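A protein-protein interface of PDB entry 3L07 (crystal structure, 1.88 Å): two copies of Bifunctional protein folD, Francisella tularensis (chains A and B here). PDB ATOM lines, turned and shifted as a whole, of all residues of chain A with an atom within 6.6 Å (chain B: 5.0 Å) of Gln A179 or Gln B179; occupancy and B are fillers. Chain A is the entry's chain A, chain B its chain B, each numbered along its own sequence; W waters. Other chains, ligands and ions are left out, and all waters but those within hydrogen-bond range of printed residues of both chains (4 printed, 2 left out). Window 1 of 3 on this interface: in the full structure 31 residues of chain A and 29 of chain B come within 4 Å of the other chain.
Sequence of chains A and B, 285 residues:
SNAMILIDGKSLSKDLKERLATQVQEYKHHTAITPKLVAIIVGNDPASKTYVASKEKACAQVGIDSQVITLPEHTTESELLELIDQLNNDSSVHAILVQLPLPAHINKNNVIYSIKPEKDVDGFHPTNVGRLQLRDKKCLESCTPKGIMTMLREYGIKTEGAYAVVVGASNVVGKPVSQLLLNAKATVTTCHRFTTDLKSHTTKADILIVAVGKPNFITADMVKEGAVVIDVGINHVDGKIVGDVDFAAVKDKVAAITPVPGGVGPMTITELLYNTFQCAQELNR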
ATOM      1  N   VAL A 129      33.795   0.498 -13.515  1.00  0.00           N
ATOM      2  CA  VAL A 129      33.460   1.800 -14.029  1.00  0.00           C
ATOM      3  C   VAL A 129      32.996   1.718 -15.524  1.00  0.00           C
ATOM      4  O   VAL A 129      31.971   2.308 -15.882  1.00  0.00           O
ATOM      5  CB  VAL A 129      34.616   2.828 -13.832  1.00  0.00           C
ATOM      6  CG1 VAL A 129      34.222   4.241 -14.339  1.00  0.00           C
ATOM      7  CG2 VAL A 129      35.011   2.965 -12.360  1.00  0.00           C
ATOM      8  N   LEU A 132      29.594  -0.035 -15.980  1.00  0.00           N
ATOM      9  CA  LEU A 132      28.434   0.784 -15.610  1.00  0.00           C
ATOM     10  C   LEU A 132      27.988   1.607 -16.833  1.00  0.00           C
ATOM     11  O   LEU A 132      26.854   1.575 -17.232  1.00  0.00           O
ATOM     12  CB  LEU A 132      28.785   1.657 -14.426  1.00  0.00           C
ATOM     13  CG  LEU A 132      27.651   2.504 -13.796  1.00  0.00           C
ATOM     14  CD1 LEU A 132      28.135   3.030 -12.467  1.00  0.00           C
ATOM     15  CD2 LEU A 132      27.355   3.622 -14.704  1.00  0.00           C
ATOM     16  N   GLN A 133      28.946   2.245 -17.476  1.00  0.00           N
ATOM     17  CA  GLN A 133      28.678   3.017 -18.697  1.00  0.00           C
ATOM     18  C   GLN A 133      28.173   2.156 -19.838  1.00  0.00           C
ATOM     19  O   GLN A 133      27.360   2.595 -20.648  1.00  0.00           O
ATOM     20  CB  GLN A 133      29.977   3.733 -19.068  1.00  0.00           C
ATOM     21  CG  GLN A 133      29.837   4.938 -19.863  1.00  0.00           C
ATOM     22  CD  GLN A 133      31.170   5.488 -20.181  1.00  0.00           C
ATOM     23  OE1 GLN A 133      31.572   5.555 -21.330  1.00  0.00           O
ATOM     24  NE2 GLN A 133      31.910   5.816 -19.134  1.00  0.00           N
ATOM     25  N   ARG A 135      26.376  -0.563 -19.480  1.00  0.00           N
ATOM     26  CA  ARG A 135      25.100  -1.261 -19.217  1.00  0.00           C
ATOM     27  C   ARG A 135      25.325  -2.737 -19.134  1.00  0.00           C
ATOM     28  O   ARG A 135      24.436  -3.477 -19.529  1.00  0.00           O
ATOM     29  CB  ARG A 135      24.066  -1.088 -20.374  1.00  0.00           C
ATOM     30  CG  ARG A 135      24.001   0.268 -20.959  1.00  0.00           C
ATOM     31  CD  ARG A 135      23.722   1.163 -19.892  1.00  0.00           C
ATOM     32  NE  ARG A 135      22.485   0.764 -19.218  1.00  0.00           N
ATOM     33  CZ  ARG A 135      21.267   1.056 -19.675  1.00  0.00           C
ATOM     34  NH1 ARG A 135      21.141   1.754 -20.795  1.00  0.00           N
ATOM     35  NH2 ARG A 135      20.177   0.668 -19.009  1.00  0.00           N
ATOM     36  N   GLY A 174      30.132  11.965  -8.545  1.00  0.00           N
ATOM     37  CA  GLY A 174      29.512  12.735  -9.593  1.00  0.00           C
ATOM     38  C   GLY A 174      29.502  12.100 -10.972  1.00  0.00           C
ATOM     39  O   GLY A 174      28.453  12.047 -11.635  1.00  0.00           O
ATOM     40  N   LYS A 175      30.621  11.541 -11.388  1.00  0.00           N
ATOM     41  CA  LYS A 175      30.644  10.905 -12.689  1.00  0.00           C
ATOM     42  C   LYS A 175      29.803   9.632 -12.715  1.00  0.00           C
ATOM     43  O   LYS A 175      28.987   9.475 -13.591  1.00  0.00           O
ATOM     44  CB  LYS A 175      32.076  10.635 -13.106  1.00  0.00           C
ATOM     45  CG  LYS A 175      32.867  11.883 -13.369  1.00  0.00           C
ATOM     46  CD  LYS A 175      34.215  11.599 -14.001  1.00  0.00           C
ATOM     47  CE  LYS A 175      35.000  12.825 -14.334  1.00  0.00           C
ATOM     48  NZ  LYS A 175      36.427  12.382 -14.619  1.00  0.00           N
ATOM     49  N   PRO A 176      29.965   8.707 -11.752  1.00  0.00           N
ATOM     50  CA  PRO A 176      29.119   7.471 -11.867  1.00  0.00           C
ATOM     51  C   PRO A 176      27.622   7.746 -11.740  1.00  0.00           C
ATOM     52  O   PRO A 176      26.814   7.097 -12.411  1.00  0.00           O
ATOM     53  CB  PRO A 176      29.613   6.584 -10.707  1.00  0.00           C
ATOM     54  CG  PRO A 176      30.506   7.437  -9.949  1.00  0.00           C
ATOM     55  CD  PRO A 176      31.059   8.493 -10.791  1.00  0.00           C
ATOM     56  N   VAL A 177      27.239   8.676 -10.877  1.00  0.00           N
ATOM     57  CA  VAL A 177      25.834   8.985 -10.744  1.00  0.00           C
ATOM     58  C   VAL A 177      25.278   9.604 -12.005  1.00  0.00           C
ATOM     59  O   VAL A 177      24.155   9.322 -12.370  1.00  0.00           O
ATOM     60  CB  VAL A 177      25.454   9.769  -9.467  1.00  0.00           C
ATOM     61  CG1 VAL A 177      25.633  11.271  -9.623  1.00  0.00           C
ATOM     62  CG2 VAL A 177      23.948   9.433  -9.074  1.00  0.00           C
ATOM     63  N   SER A 178      26.050  10.404 -12.714  1.00  0.00           N
ATOM     64  CA  SER A 178      25.603  10.964 -13.941  1.00  0.00           C
ATOM     65  C   SER A 178      25.353   9.830 -14.948  1.00  0.00           C
ATOM     66  O   SER A 178      24.438   9.911 -15.768  1.00  0.00           O
ATOM     67  CB  SER A 178      26.668  11.900 -14.514  1.00  0.00           C
ATOM     68  OG  SER A 178      26.915  13.016 -13.626  1.00  0.00           O
ATOM     69  N   GLN A 179      26.237   8.846 -14.949  1.00  0.00           N
ATOM     70  CA  GLN A 179      26.115   7.748 -15.900  1.00  0.00           C
ATOM     71  C   GLN A 179      24.889   6.885 -15.579  1.00  0.00           C
ATOM     72  O   GLN A 179      24.188   6.411 -16.527  1.00  0.00           O
ATOM     73  CB  GLN A 179      27.385   6.893 -15.956  1.00  0.00           C
ATOM     74  CG  GLN A 179      28.584   7.596 -16.546  1.00  0.00           C
ATOM     75  CD  GLN A 179      28.272   8.206 -17.874  1.00  0.00           C
ATOM     76  OE1 GLN A 179      27.863   7.524 -18.779  1.00  0.00           O
ATOM     77  NE2 GLN A 179      28.352   9.521 -17.960  1.00  0.00           N
ATOM     78  N   LEU A 180      24.640   6.664 -14.288  1.00  0.00           N
ATOM     79  CA  LEU A 180      23.443   5.932 -13.882  1.00  0.00           C
ATOM     80  C   LEU A 180      22.155   6.697 -14.325  1.00  0.00           C
ATOM     81  O   LEU A 180      21.176   6.093 -14.768  1.00  0.00           O
ATOM     82  CB  LEU A 180      23.443   5.721 -12.382  1.00  0.00           C
ATOM     83  CG  LEU A 180      24.485   4.673 -11.895  1.00  0.00           C
ATOM     84  CD1 LEU A 180      24.553   4.578 -10.368  1.00  0.00           C
ATOM     85  CD2 LEU A 180      24.212   3.239 -12.468  1.00  0.00           C
ATOM     86  N   LEU A 181      22.167   8.003 -14.159  1.00  0.00           N
ATOM     87  CA  LEU A 181      21.021   8.835 -14.524  1.00  0.00           C
ATOM     88  C   LEU A 181      20.791   8.776 -16.018  1.00  0.00           C
ATOM     89  O   LEU A 181      19.653   8.668 -16.444  1.00  0.00           O
ATOM     90  CB  LEU A 181      21.217  10.274 -14.067  1.00  0.00           C
ATOM     91  CG  LEU A 181      21.036  10.459 -12.540  1.00  0.00           C
ATOM     92  CD1 LEU A 181      21.608  11.778 -12.020  1.00  0.00           C
ATOM     93  CD2 LEU A 181      19.550  10.338 -12.224  1.00  0.00           C
ATOM     94  N   LEU A 182      21.870   8.805 -16.788  1.00  0.00           N
ATOM     95  CA  LEU A 182      21.745   8.696 -18.248  1.00  0.00           C
ATOM     96  C   LEU A 182      21.173   7.327 -18.609  1.00  0.00           C
ATOM     97  O   LEU A 182      20.292   7.248 -19.477  1.00  0.00           O
ATOM     98  CB  LEU A 182      23.097   8.897 -18.959  1.00  0.00           C
ATOM     99  CG  LEU A 182      23.611  10.290 -19.309  1.00  0.00           C
ATOM    100  CD1 LEU A 182      25.095  10.282 -19.734  1.00  0.00           C
ATOM    101  CD2 LEU A 182      22.656  10.890 -20.411  1.00  0.00           C
ATOM    102  N   ASN A 183      21.640   6.254 -17.957  1.00  0.00           N
ATOM    103  CA  ASN A 183      21.129   4.900 -18.211  1.00  0.00           C
ATOM    104  C   ASN A 183      19.648   4.785 -17.853  1.00  0.00           C
ATOM    105  O   ASN A 183      18.894   3.995 -18.489  1.00  0.00           O
ATOM    106  CB  ASN A 183      21.929   3.824 -17.434  1.00  0.00           C
ATOM    107  CG  ASN A 183      23.315   3.604 -18.000  1.00  0.00           C
ATOM    108  OD1 ASN A 183      23.602   3.972 -19.126  1.00  0.00           O
ATOM    109  ND2 ASN A 183      24.148   2.901 -17.237  1.00  0.00           N
ATOM    110  N   ALA A 184      19.211   5.610 -16.888  1.00  0.00           N
ATOM    111  CA  ALA A 184      17.835   5.688 -16.442  1.00  0.00           C
ATOM    112  C   ALA A 184      17.005   6.662 -17.341  1.00  0.00           C
ATOM    113  O   ALA A 184      15.894   6.994 -17.034  1.00  0.00           O
ATOM    114  CB  ALA A 184      17.786   6.165 -14.924  1.00  0.00           C
ATOM    115  N   VAL A 188      21.286  14.584 -18.748  1.00  0.00           N
ATOM    116  CA  VAL A 188      22.166  14.862 -17.612  1.00  0.00           C
ATOM    117  C   VAL A 188      23.209  15.887 -17.954  1.00  0.00           C
ATOM    118  O   VAL A 188      23.926  15.736 -18.934  1.00  0.00           O
ATOM    119  CB  VAL A 188      22.887  13.540 -17.156  1.00  0.00           C
ATOM    120  CG1 VAL A 188      23.727  13.804 -15.876  1.00  0.00           C
ATOM    121  CG2 VAL A 188      21.835  12.453 -16.915  1.00  0.00           C
ATOM    122  N   THR A 190      26.647  17.568 -16.191  1.00  0.00           N
ATOM    123  CA  THR A 190      27.615  17.449 -15.136  1.00  0.00           C
ATOM    124  C   THR A 190      28.418  18.783 -15.046  1.00  0.00           C
ATOM    125  O   THR A 190      29.058  19.236 -16.029  1.00  0.00           O
ATOM    126  CB  THR A 190      28.532  16.237 -15.315  1.00  0.00           C
ATOM    127  OG1 THR A 190      27.775  15.028 -15.438  1.00  0.00           O
ATOM    128  CG2 THR A 190      29.487  16.137 -14.100  1.00  0.00           C
ATOM    129  N   LEU B 132      39.323   5.883 -19.068  1.00  0.00           N
ATOM    130  CA  LEU B 132      38.973   7.149 -19.713  1.00  0.00           C
ATOM    131  C   LEU B 132      38.303   8.066 -18.678  1.00  0.00           C
ATOM    132  O   LEU B 132      38.763   9.165 -18.439  1.00  0.00           O
ATOM    133  CB  LEU B 132      38.077   6.933 -20.926  1.00  0.00           C
ATOM    134  CG  LEU B 132      37.870   8.159 -21.811  1.00  0.00           C
ATOM    135  CD1 LEU B 132      37.619   7.722 -23.287  1.00  0.00           C
ATOM    136  CD2 LEU B 132      36.771   9.014 -21.326  1.00  0.00           C
ATOM    137  N   GLN B 133      37.259   7.554 -18.047  1.00  0.00           N
ATOM    138  CA  GLN B 133      36.425   8.323 -17.091  1.00  0.00           C
ATOM    139  C   GLN B 133      37.329   8.682 -15.927  1.00  0.00           C
ATOM    140  O   GLN B 133      37.413   9.836 -15.547  1.00  0.00           O
ATOM    141  CB  GLN B 133      35.181   7.493 -16.711  1.00  0.00           C
ATOM    142  CG  GLN B 133      34.323   7.990 -15.525  1.00  0.00           C
ATOM    143  CD  GLN B 133      33.034   7.260 -15.397  1.00  0.00           C
ATOM    144  OE1 GLN B 133      32.533   6.728 -16.396  1.00  0.00           O
ATOM    145  NE2 GLN B 133      32.462   7.215 -14.198  1.00  0.00           N
ATOM    146  N   LYS B 175      28.801   8.722 -25.182  1.00  0.00           N
ATOM    147  CA  LYS B 175      29.187   8.694 -23.773  1.00  0.00           C
ATOM    148  C   LYS B 175      30.710   8.896 -23.608  1.00  0.00           C
ATOM    149  O   LYS B 175      31.105   9.684 -22.793  1.00  0.00           O
ATOM    150  CB  LYS B 175      28.776   7.407 -23.067  1.00  0.00           C
ATOM    151  CG  LYS B 175      27.279   7.242 -22.974  1.00  0.00           C
ATOM    152  CD  LYS B 175      26.961   6.202 -21.915  1.00  0.00           C
ATOM    153  CE  LYS B 175      25.930   5.289 -22.347  1.00  0.00           C
ATOM    154  NZ  LYS B 175      25.440   4.390 -21.341  1.00  0.00           N
ATOM    155  N   PRO B 176      31.543   8.220 -24.432  1.00  0.00           N
ATOM    156  CA  PRO B 176      32.962   8.551 -24.236  1.00  0.00           C
ATOM    157  C   PRO B 176      33.363   9.981 -24.598  1.00  0.00           C
ATOM    158  O   PRO B 176      34.194  10.554 -23.874  1.00  0.00           O
ATOM    159  CB  PRO B 176      33.686   7.557 -25.113  1.00  0.00           C
ATOM    160  CG  PRO B 176      32.649   6.900 -25.902  1.00  0.00           C
ATOM    161  CD  PRO B 176      31.363   7.021 -25.266  1.00  0.00           C
ATOM    162  N   VAL B 177      32.802  10.577 -25.639  1.00  0.00           N
ATOM    163  CA  VAL B 177      33.127  11.958 -25.929  1.00  0.00           C
ATOM    164  C   VAL B 177      32.667  12.915 -24.801  1.00  0.00           C
ATOM    165  O   VAL B 177      33.384  13.866 -24.503  1.00  0.00           O
ATOM    166  CB  VAL B 177      32.745  12.446 -27.360  1.00  0.00           C
ATOM    167  CG1 VAL B 177      31.299  12.894 -27.394  1.00  0.00           C
ATOM    168  CG2 VAL B 177      33.678  13.551 -27.828  1.00  0.00           C
ATOM    169  N   SER B 178      31.529  12.655 -24.156  1.00  0.00           N
ATOM    170  CA  SER B 178      31.064  13.435 -23.048  1.00  0.00           C
ATOM    171  C   SER B 178      32.062  13.348 -21.919  1.00  0.00           C
ATOM    172  O   SER B 178      32.392  14.360 -21.315  1.00  0.00           O
ATOM    173  CB  SER B 178      29.682  12.997 -22.529  1.00  0.00           C
ATOM    174  OG  SER B 178      28.711  13.128 -23.583  1.00  0.00           O
ATOM    175  N   GLN B 179      32.568  12.178 -21.652  1.00  0.00           N
ATOM    176  CA  GLN B 179      33.632  12.020 -20.656  1.00  0.00           C
ATOM    177  C   GLN B 179      34.985  12.725 -21.020  1.00  0.00           C
ATOM    178  O   GLN B 179      35.582  13.303 -20.133  1.00  0.00           O
ATOM    179  CB  GLN B 179      33.883  10.529 -20.293  1.00  0.00           C
ATOM    180  CG  GLN B 179      32.611   9.877 -19.619  1.00  0.00           C
ATOM    181  CD  GLN B 179      32.136  10.656 -18.399  1.00  0.00           C
ATOM    182  OE1 GLN B 179      32.889  10.920 -17.486  1.00  0.00           O
ATOM    183  NE2 GLN B 179      30.878  11.103 -18.434  1.00  0.00           N
ATOM    184  N   LEU B 180      35.412  12.661 -22.271  1.00  0.00           N
ATOM    185  CA  LEU B 180      36.588  13.392 -22.711  1.00  0.00           C
ATOM    186  C   LEU B 180      36.423  14.897 -22.548  1.00  0.00           C
ATOM    187  O   LEU B 180      37.321  15.548 -22.098  1.00  0.00           O
ATOM    188  CB  LEU B 180      36.914  13.039 -24.127  1.00  0.00           C
ATOM    189  CG  LEU B 180      37.478  11.629 -24.325  1.00  0.00           C
ATOM    190  CD1 LEU B 180      37.622  11.291 -25.798  1.00  0.00           C
ATOM    191  CD2 LEU B 180      38.792  11.362 -23.574  1.00  0.00           C
ATOM    192  N   LEU B 181      35.251  15.416 -22.892  1.00  0.00           N
ATOM    193  CA  LEU B 181      34.909  16.842 -22.745  1.00  0.00           C
ATOM    194  C   LEU B 181      34.934  17.274 -21.285  1.00  0.00           C
ATOM    195  O   LEU B 181      35.476  18.332 -20.918  1.00  0.00           O
ATOM    196  CB  LEU B 181      33.580  17.165 -23.433  1.00  0.00           C
ATOM    197  CG  LEU B 181      33.756  17.261 -24.950  1.00  0.00           C
ATOM    198  CD1 LEU B 181      32.358  17.104 -25.659  1.00  0.00           C
ATOM    199  CD2 LEU B 181      34.428  18.601 -25.426  1.00  0.00           C
ATOM    200  N   LEU B 182      34.431  16.411 -20.428  1.00  0.00           N
ATOM    201  CA  LEU B 182      34.366  16.718 -19.022  1.00  0.00           C
ATOM    202  C   LEU B 182      35.809  16.727 -18.463  1.00  0.00           C
ATOM    203  O   LEU B 182      36.124  17.580 -17.676  1.00  0.00           O
ATOM    204  CB  LEU B 182      33.529  15.646 -18.300  1.00  0.00           C
ATOM    205  CG  LEU B 182      32.857  15.890 -16.990  1.00  0.00           C
ATOM    206  CD1 LEU B 182      31.903  17.114 -17.063  1.00  0.00           C
ATOM    207  CD2 LEU B 182      32.094  14.512 -16.499  1.00  0.00           C
ATOM    208  N   ASN B 183      36.654  15.771 -18.867  1.00  0.00           N
ATOM    209  CA  ASN B 183      38.074  15.769 -18.456  1.00  0.00           C
ATOM    210  C   ASN B 183      38.783  17.016 -18.958  1.00  0.00           C
ATOM    211  O   ASN B 183      39.696  17.518 -18.308  1.00  0.00           O
ATOM    212  CB  ASN B 183      38.807  14.512 -18.957  1.00  0.00           C
ATOM    213  CG  ASN B 183      38.300  13.250 -18.273  1.00  0.00           C
ATOM    214  OD1 ASN B 183      37.629  13.360 -17.288  1.00  0.00           O
ATOM    215  ND2 ASN B 183      38.658  12.062 -18.793  1.00  0.00           N
HETATM  216  O   HOH W   1      29.475  12.789 -16.537  1.00  0.00           O
HETATM  217  O   HOH W   2      30.808   4.776 -15.727  1.00  0.00           O
HETATM  218  O   HOH W   3      29.066   9.770 -20.475  1.00  0.00           O
HETATM  219  O   HOH W   4      26.023   5.779 -18.777  1.00  0.00           O
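The side-chain amide oxygen (OD1) of Asn B183 is in hydrogen-bond range of the side-chain amino group (NZ) of Lys A175 (3.1 Å).
The backbone carbonyl oxygen (O) of Gln A133 lies within hydrogen-bond range of the side-chain amino group (NZ) of Lys B175, 2.7 Å away.
NZ of Lys A175 is in hydrogen-bond range of O of Gln B133, at 2.9 Å.
The side-chain amide nitrogen (NE2) of Gln A179 sits close to the side-chain amide nitrogen (NE2) of Gln B179 (3.0 Å).
The side-chain amide nitrogen (NE2) of Gln A133 is in hydrogen-bond range of the side-chain amide oxygen (OE1) of Gln B133, at 3.0 Å.
The side-chain amide oxygen of Asn A183 lies within hydrogen-bond range of the side-chain amino group of Lys B175 (2.9 Å).
Of the 11 printed residues of chain B, 5 touch a printed residue of chain A.
Printed residues of chain B that touch a printed residue of chain A: Gln B133, Lys B175, Gln B179, Leu B182 and Asn B183.
Printed residues of chain A that touch a printed residue of chain B: Val A129, Gln A133, Arg A135, Lys A175, Pro A176, Gln A179, Asn A183 and Thr A190.
Lys A175 touches Gln B179, and with the chains exchanged Gln A179 touches Lys B175.
Lys A175 touches Leu B182, but with the chains exchanged Leu A182 does not touch Lys B175 (5.0 Å).
Lys A175 touches Asn B183, and with the chains exchanged Asn A183 touches Lys B175.
Gln A179 touches its own counterpart, Gln B179.
11 positions are printed for both chains.
Of the 13 pairs that touch across the chains among the printed residues, 8 have their exchanged pair printed and touching as well.
Among the printed residues, merely in contact across the chains: Val A129 with Gln B133 (3.4 Å), Gln A179 with Lys B175 (3.5 Å), Thr A190 with Leu B182 (3.7 Å), Lys A175 with Gln B179 (3.8 Å), Pro A176 with Gln B133 (3.8 Å), Arg A135 with Lys B175 (3.9 Å) and Lys A175 with Leu B182 (3.997 Å).
O of Leu B132 is in hydrogen-bond range of ND2 of Asn B183 (2.9 Å).
The guanidinium group of Arg A135 sits close to the side-chain amide nitrogen of Asn A183, 3.4 Å away.
The side-chain hydroxyl of Ser A178 sits at hydrogen-bond distance from the side-chain hydroxyl of Thr A190 (2.8 Å).
O of Leu A132 is in hydrogen-bond range of ND2 of Asn A183 (3.0 Å).
Of the printed residues of chain B, Gln A179 touches Lys B175 and Gln B179.
Printed residues of chain B within 4 Å of Arg A135: Lys B175.
Of the printed residues of chain A, Gln B133 touches Val A129, Gln A133, Lys A175 and Pro A176.
Of the printed residues of chain B, Pro A176 touches Gln B133.
Val A188 touches none of the printed residues of chain B.
Ser B178 touches none of the printed residues of chain A.
The nearest residue of chain B that does not touch Gln A179 is Gln B133 (4.05 Å).
Water W4 lies within hydrogen-bond range of the side-chain amide oxygen of Gln A179 (2.5 Å), the side-chain amino group of Lys B175 (3.0 Å) and the side-chain amide oxygen of Asn A183 (3.0 Å).
Water W3 lies within hydrogen-bond range of NE2 of Gln A179, NE2 of Gln B179 and O of Lys B175.
Water W2 lies within hydrogen-bond range of OE1 of Gln B133 (2.7 Å) and O of Val A129 (2.7 Å).
Water W1 lies within hydrogen-bond range of NE2 of Gln B179 (2.9 Å) and OG1 of Thr A190 (3.0 Å).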
